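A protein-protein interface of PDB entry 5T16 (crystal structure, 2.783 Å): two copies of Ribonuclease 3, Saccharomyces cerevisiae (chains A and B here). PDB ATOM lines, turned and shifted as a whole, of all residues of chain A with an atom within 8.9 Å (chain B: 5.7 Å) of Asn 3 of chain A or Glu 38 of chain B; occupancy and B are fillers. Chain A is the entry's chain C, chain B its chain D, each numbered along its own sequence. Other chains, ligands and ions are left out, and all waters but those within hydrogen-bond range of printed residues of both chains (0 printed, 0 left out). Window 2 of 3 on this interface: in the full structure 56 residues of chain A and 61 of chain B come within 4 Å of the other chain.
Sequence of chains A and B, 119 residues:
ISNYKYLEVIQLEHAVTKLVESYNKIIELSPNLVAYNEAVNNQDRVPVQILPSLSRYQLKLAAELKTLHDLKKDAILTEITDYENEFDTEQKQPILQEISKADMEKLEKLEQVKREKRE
Hydrophobic or aromatic side chains of chain B that line the printed part of chain A: Tyr 36 and Ala 39. Of the 10 printed residues of chain A, 2 touch a printed residue of chain B. Among the printed residues, no Asp or Glu carboxylate lies within 4 Å of a Lys or Arg side-chain nitrogen of the other chain.
No position is printed for both chains.
ND2 of Asn 3 of chain A lies within hydrogen-bond range of OE1 of Glu 38 of chain B, at 3.0 Å.
Printed residues of chain B within 4 Å of Asn 3 of chain A: Glu 38. Printed residues of chain B within 4 Å of Tyr 4 of chain A: Tyr 36 and Ala 39. Of the printed residues of chain A, Tyr 36 of chain B touches Tyr 4 (3.7 Å). Printed residues of chain A within 4 Å of Glu 38 of chain B: Asn 3. Ala 39 of chain B touches just one residue of chain A: Tyr 4 (3.9 Å). The nearest printed residue of chain B that does not touch Asn 3 of chain A is Ala 35 of chain B (4.0002 Å). The nearest residue of chain A that does not touch Glu 38 of chain B is Tyr 4 of chain A (7.2 Å).
Among the printed residues, pairs that only touch across the chains: Tyr 4 of chain A with Tyr 36 of chain B and Tyr 4 of chain A with Ala 39 of chain B.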
ATOM      1  N   SER A   2      20.477 -13.806  38.545  1.00  0.00           N
ATOM      2  CA  SER A   2      20.951 -14.309  37.256  1.00  0.00           C
ATOM      3  C   SER A   2      20.103 -13.939  36.045  1.00  0.00           C
ATOM      4  O   SER A   2      18.885 -13.741  36.105  1.00  0.00           O
ATOM      5  CB  SER A   2      21.106 -15.846  37.273  1.00  0.00           C
ATOM      6  OG  SER A   2      22.107 -16.268  38.187  1.00  0.00           O
ATOM      7  N   ASN A   3      20.817 -13.959  34.937  1.00  0.00           N
ATOM      8  CA  ASN A   3      20.338 -13.677  33.618  1.00  0.00           C
ATOM      9  C   ASN A   3      19.452 -14.763  33.064  1.00  0.00           C
ATOM     10  O   ASN A   3      18.286 -14.543  32.841  1.00  0.00           O
ATOM     11  CB  ASN A   3      21.518 -13.520  32.656  1.00  0.00           C
ATOM     12  CG  ASN A   3      22.771 -12.989  33.321  1.00  0.00           C
ATOM     13  OD1 ASN A   3      22.821 -12.847  34.532  1.00  0.00           O
ATOM     14  ND2 ASN A   3      23.788 -12.708  32.529  1.00  0.00           N
ATOM     15  N   TYR A   4      20.032 -15.929  32.822  1.00  0.00           N
ATOM     16  CA  TYR A   4      19.331 -17.074  32.258  1.00  0.00           C
ATOM     17  C   TYR A   4      18.824 -18.003  33.370  1.00  0.00           C
ATOM     18  O   TYR A   4      19.538 -18.245  34.342  1.00  0.00           O
ATOM     19  CB  TYR A   4      20.270 -17.833  31.312  1.00  0.00           C
ATOM     20  CG  TYR A   4      20.432 -17.241  29.908  1.00  0.00           C
ATOM     21  CD1 TYR A   4      19.507 -17.481  28.896  1.00  0.00           C
ATOM     22  CD2 TYR A   4      21.512 -16.413  29.608  1.00  0.00           C
ATOM     23  CE1 TYR A   4      19.675 -16.930  27.619  1.00  0.00           C
ATOM     24  CE2 TYR A   4      21.673 -15.851  28.347  1.00  0.00           C
ATOM     25  CZ  TYR A   4      20.758 -16.115  27.360  1.00  0.00           C
ATOM     26  OH  TYR A   4      20.939 -15.548  26.120  1.00  0.00           O
ATOM     27  N   LYS A   5      17.581 -18.469  33.258  1.00  0.00           N
ATOM     28  CA  LYS A   5      17.013 -19.458  34.180  1.00  0.00           C
ATOM     29  C   LYS A   5      16.693 -20.700  33.362  1.00  0.00           C
ATOM     30  O   LYS A   5      16.401 -20.584  32.169  1.00  0.00           O
ATOM     31  CB  LYS A   5      15.747 -18.952  34.882  1.00  0.00           C
ATOM     32  CG  LYS A   5      15.895 -17.672  35.682  1.00  0.00           C
ATOM     33  CD  LYS A   5      16.621 -17.940  36.987  1.00  0.00           C
ATOM     34  CE  LYS A   5      16.185 -16.943  38.059  1.00  0.00           C
ATOM     35  NZ  LYS A   5      16.810 -17.240  39.388  1.00  0.00           N
ATOM     36  N   TYR A   6      16.764 -21.882  33.975  1.00  0.00           N
ATOM     37  CA  TYR A   6      16.572 -23.122  33.227  1.00  0.00           C
ATOM     38  C   TYR A   6      15.229 -23.056  32.498  1.00  0.00           C
ATOM     39  O   TYR A   6      15.146 -23.306  31.300  1.00  0.00           O
ATOM     40  CB  TYR A   6      16.642 -24.351  34.132  1.00  0.00           C
ATOM     41  CG  TYR A   6      16.588 -25.666  33.357  1.00  0.00           C
ATOM     42  CD1 TYR A   6      17.565 -25.990  32.428  1.00  0.00           C
ATOM     43  CD2 TYR A   6      15.574 -26.585  33.564  1.00  0.00           C
ATOM     44  CE1 TYR A   6      17.527 -27.174  31.724  1.00  0.00           C
ATOM     45  CE2 TYR A   6      15.532 -27.780  32.858  1.00  0.00           C
ATOM     46  CZ  TYR A   6      16.515 -28.070  31.943  1.00  0.00           C
ATOM     47  OH  TYR A   6      16.483 -29.254  31.233  1.00  0.00           O
ATOM     48  N   GLU A   8      13.614 -20.576  31.473  1.00  0.00           N
ATOM     49  CA  GLU A   8      13.656 -19.658  30.341  1.00  0.00           C
ATOM     50  C   GLU A   8      14.398 -20.292  29.164  1.00  0.00           C
ATOM     51  O   GLU A   8      14.052 -20.086  27.997  1.00  0.00           O
ATOM     52  CB  GLU A   8      14.325 -18.342  30.728  1.00  0.00           C
ATOM     53  CG  GLU A   8      13.579 -17.539  31.784  1.00  0.00           C
ATOM     54  CD  GLU A   8      14.272 -16.223  32.170  1.00  0.00           C
ATOM     55  OE1 GLU A   8      15.517 -16.197  32.375  1.00  0.00           O
ATOM     56  OE2 GLU A   8      13.548 -15.205  32.267  1.00  0.00           O
ATOM     57  N   VAL A   9      15.413 -21.082  29.484  1.00  0.00           N
ATOM     58  CA  VAL A   9      16.280 -21.675  28.469  1.00  0.00           C
ATOM     59  C   VAL A   9      15.567 -22.709  27.594  1.00  0.00           C
ATOM     60  O   VAL A   9      15.629 -22.658  26.360  1.00  0.00           O
ATOM     61  CB  VAL A   9      17.520 -22.336  29.146  1.00  0.00           C
ATOM     62  CG1 VAL A   9      18.115 -23.337  28.250  1.00  0.00           C
ATOM     63  CG2 VAL A   9      18.574 -21.294  29.528  1.00  0.00           C
ATOM     64  N   LEU A  12      13.159 -21.228  25.218  1.00  0.00           N
ATOM     65  CA  LEU A  12      13.844 -20.505  24.151  1.00  0.00           C
ATOM     66  C   LEU A  12      14.340 -21.469  23.086  1.00  0.00           C
ATOM     67  O   LEU A  12      14.157 -21.213  21.899  1.00  0.00           O
ATOM     68  CB  LEU A  12      15.005 -19.690  24.716  1.00  0.00           C
ATOM     69  CG  LEU A  12      14.695 -18.287  25.252  1.00  0.00           C
ATOM     70  CD1 LEU A  12      15.898 -17.746  25.964  1.00  0.00           C
ATOM     71  CD2 LEU A  12      14.312 -17.345  24.145  1.00  0.00           C
ATOM     72  N   GLU A 108      26.764  -2.287  24.305  1.00  0.00           N
ATOM     73  CA  GLU A 108      27.563  -2.678  25.454  1.00  0.00           C
ATOM     74  C   GLU A 108      27.597  -1.506  26.455  1.00  0.00           C
ATOM     75  O   GLU A 108      27.366  -1.706  27.672  1.00  0.00           O
ATOM     76  CB  GLU A 108      28.971  -3.110  25.020  1.00  0.00           C
ATOM     77  CG  GLU A 108      28.960  -3.948  23.737  1.00  0.00           C
ATOM     78  CD  GLU A 108      30.341  -4.382  23.244  1.00  0.00           C
ATOM     79  OE1 GLU A 108      31.022  -3.626  22.499  1.00  0.00           O
ATOM     80  OE2 GLU A 108      30.750  -5.505  23.623  1.00  0.00           O
ATOM     81  N   GLU A 111      24.250  -1.031  28.592  1.00  0.00           N
ATOM     82  CA  GLU A 111      24.209  -1.779  29.853  1.00  0.00           C
ATOM     83  C   GLU A 111      25.488  -1.593  30.686  1.00  0.00           C
ATOM     84  O   GLU A 111      25.494  -1.869  31.894  1.00  0.00           O
ATOM     85  CB  GLU A 111      23.893  -3.275  29.647  1.00  0.00           C
ATOM     86  CG  GLU A 111      22.459  -3.560  29.152  1.00  0.00           C
ATOM     87  CD  GLU A 111      21.375  -2.951  30.105  1.00  0.00           C
ATOM     88  OE1 GLU A 111      21.605  -2.902  31.346  1.00  0.00           O
ATOM     89  OE2 GLU A 111      20.262  -2.592  29.625  1.00  0.00           O
ATOM     90  N   LEU B  33      22.404  -9.731  22.824  1.00  0.00           N
ATOM     91  CA  LEU B  33      23.677 -10.379  22.639  1.00  0.00           C
ATOM     92  C   LEU B  33      24.722 -10.068  23.728  1.00  0.00           C
ATOM     93  O   LEU B  33      25.667 -10.843  23.934  1.00  0.00           O
ATOM     94  CB  LEU B  33      24.205 -10.001  21.262  1.00  0.00           C
ATOM     95  CG  LEU B  33      25.224 -10.979  20.701  1.00  0.00           C
ATOM     96  CD1 LEU B  33      24.672 -12.389  20.780  1.00  0.00           C
ATOM     97  CD2 LEU B  33      25.513 -10.598  19.272  1.00  0.00           C
ATOM     98  N   VAL B  34      24.567  -8.952  24.433  1.00  0.00           N
ATOM     99  CA  VAL B  34      25.536  -8.640  25.472  1.00  0.00           C
ATOM    100  C   VAL B  34      25.350  -9.576  26.660  1.00  0.00           C
ATOM    101  O   VAL B  34      26.331 -10.088  27.194  1.00  0.00           O
ATOM    102  CB  VAL B  34      25.496  -7.153  25.906  1.00  0.00           C
ATOM    103  CG1 VAL B  34      25.575  -6.240  24.681  1.00  0.00           C
ATOM    104  CG2 VAL B  34      24.300  -6.826  26.802  1.00  0.00           C
ATOM    105  N   ALA B  35      24.107  -9.809  27.073  1.00  0.00           N
ATOM    106  CA  ALA B  35      23.852 -10.710  28.183  1.00  0.00           C
ATOM    107  C   ALA B  35      24.218 -12.141  27.792  1.00  0.00           C
ATOM    108  O   ALA B  35      24.665 -12.923  28.632  1.00  0.00           O
ATOM    109  CB  ALA B  35      22.418 -10.627  28.636  1.00  0.00           C
ATOM    110  N   TYR B  36      24.024 -12.489  26.525  1.00  0.00           N
ATOM    111  CA  TYR B  36      24.435 -13.808  26.047  1.00  0.00           C
ATOM    112  C   TYR B  36      25.935 -14.007  26.168  1.00  0.00           C
ATOM    113  O   TYR B  36      26.390 -15.025  26.689  1.00  0.00           O
ATOM    114  CB  TYR B  36      24.003 -14.026  24.600  1.00  0.00           C
ATOM    115  CG  TYR B  36      24.541 -15.306  24.007  1.00  0.00           C
ATOM    116  CD1 TYR B  36      23.923 -16.521  24.246  1.00  0.00           C
ATOM    117  CD2 TYR B  36      25.667 -15.295  23.191  1.00  0.00           C
ATOM    118  CE1 TYR B  36      24.419 -17.698  23.699  1.00  0.00           C
ATOM    119  CE2 TYR B  36      26.172 -16.463  22.639  1.00  0.00           C
ATOM    120  CZ  TYR B  36      25.543 -17.665  22.897  1.00  0.00           C
ATOM    121  OH  TYR B  36      26.032 -18.829  22.352  1.00  0.00           O
ATOM    122  N   ASN B  37      26.686 -13.039  25.647  1.00  0.00           N
ATOM    123  CA  ASN B  37      28.145 -13.076  25.669  1.00  0.00           C
ATOM    124  C   ASN B  37      28.708 -13.137  27.081  1.00  0.00           C
ATOM    125  O   ASN B  37      29.693 -13.835  27.337  1.00  0.00           O
ATOM    126  CB  ASN B  37      28.718 -11.860  24.938  1.00  0.00           C
ATOM    127  CG  ASN B  37      28.755 -12.039  23.427  1.00  0.00           C
ATOM    128  OD1 ASN B  37      28.956 -13.152  22.912  1.00  0.00           O
ATOM    129  ND2 ASN B  37      28.531 -10.942  22.702  1.00  0.00           N
ATOM    130  N   GLU B  38      28.099 -12.397  28.000  1.00  0.00           N
ATOM    131  CA  GLU B  38      28.571 -12.440  29.372  1.00  0.00           C
ATOM    132  C   GLU B  38      28.350 -13.835  29.940  1.00  0.00           C
ATOM    133  O   GLU B  38      29.243 -14.422  30.556  1.00  0.00           O
ATOM    134  CB  GLU B  38      27.872 -11.378  30.227  1.00  0.00           C
ATOM    135  CG  GLU B  38      28.184 -11.473  31.712  1.00  0.00           C
ATOM    136  CD  GLU B  38      27.330 -10.543  32.558  1.00  0.00           C
ATOM    137  OE1 GLU B  38      26.154 -10.873  32.806  1.00  0.00           O
ATOM    138  OE2 GLU B  38      27.840  -9.478  32.978  1.00  0.00           O
ATOM    139  N   ALA B  39      27.182 -14.399  29.663  1.00  0.00           N
ATOM    140  CA  ALA B  39      26.847 -15.694  30.219  1.00  0.00           C
ATOM    141  C   ALA B  39      27.729 -16.783  29.618  1.00  0.00           C
ATOM    142  O   ALA B  39      28.223 -17.652  30.334  1.00  0.00           O
ATOM    143  CB  ALA B  39      25.386 -16.000  29.996  1.00  0.00           C
ATOM    144  N   VAL B  40      27.944 -16.727  28.309  1.00  0.00           N
ATOM    145  CA  VAL B  40      28.702 -17.781  27.649  1.00  0.00           C
ATOM    146  C   VAL B  40      30.180 -17.678  28.087  1.00  0.00           C
ATOM    147  O   VAL B  40      30.914 -18.672  28.058  1.00  0.00           O
ATOM    148  CB  VAL B  40      28.531 -17.727  26.093  1.00  0.00           C
ATOM    149  CG1 VAL B  40      29.134 -16.475  25.516  1.00  0.00           C
ATOM    150  CG2 VAL B  40      29.165 -18.931  25.436  1.00  0.00           C
ATOM    151  N   ASN B  41      30.618 -16.473  28.466  1.00  0.00           N
ATOM    152  CA  ASN B  41      31.999 -16.259  28.939  1.00  0.00           C
ATOM    153  C   ASN B  41      32.276 -16.489  30.436  1.00  0.00           C
ATOM    154  O   ASN B  41      33.432 -16.664  30.817  1.00  0.00           O
ATOM    155  CB  ASN B  41      32.459 -14.834  28.606  1.00  0.00           C
ATOM    156  CG  ASN B  41      32.700 -14.624  27.115  1.00  0.00           C
ATOM    157  OD1 ASN B  41      32.904 -15.582  26.354  1.00  0.00           O
ATOM    158  ND2 ASN B  41      32.687 -13.359  26.693  1.00  0.00           N
ATOM    159  N   ASN B  42      31.256 -16.438  31.299  1.00  0.00           N
ATOM    160  CA  ASN B  42      31.444 -16.913  32.669  1.00  0.00           C
ATOM    161  C   ASN B  42      30.485 -18.040  32.998  1.00  0.00           C
ATOM    162  O   ASN B  42      29.402 -17.787  33.511  1.00  0.00           O
ATOM    163  CB  ASN B  42      31.213 -15.767  33.661  1.00  0.00           C
ATOM    164  CG  ASN B  42      31.780 -14.436  33.179  1.00  0.00           C
ATOM    165  OD1 ASN B  42      32.627 -14.383  32.287  1.00  0.00           O
ATOM    166  ND2 ASN B  42      31.306 -13.347  33.775  1.00  0.00           N
ATOM    167  N   GLN B  43      30.903 -19.284  32.839  1.00  0.00           N
ATOM    168  CA  GLN B  43      29.912 -20.347  32.966  1.00  0.00           C
ATOM    169  C   GLN B  43      29.847 -20.992  34.345  1.00  0.00           C
ATOM    170  O   GLN B  43      28.907 -21.741  34.635  1.00  0.00           O
ATOM    171  CB  GLN B  43      30.144 -21.408  31.882  1.00  0.00           C
ATOM    172  CG  GLN B  43      29.886 -20.863  30.481  1.00  0.00           C
ATOM    173  CD  GLN B  43      29.991 -21.916  29.398  1.00  0.00           C
ATOM    174  OE1 GLN B  43      29.899 -23.115  29.667  1.00  0.00           O
ATOM    175  NE2 GLN B  43      30.203 -21.474  28.163  1.00  0.00           N
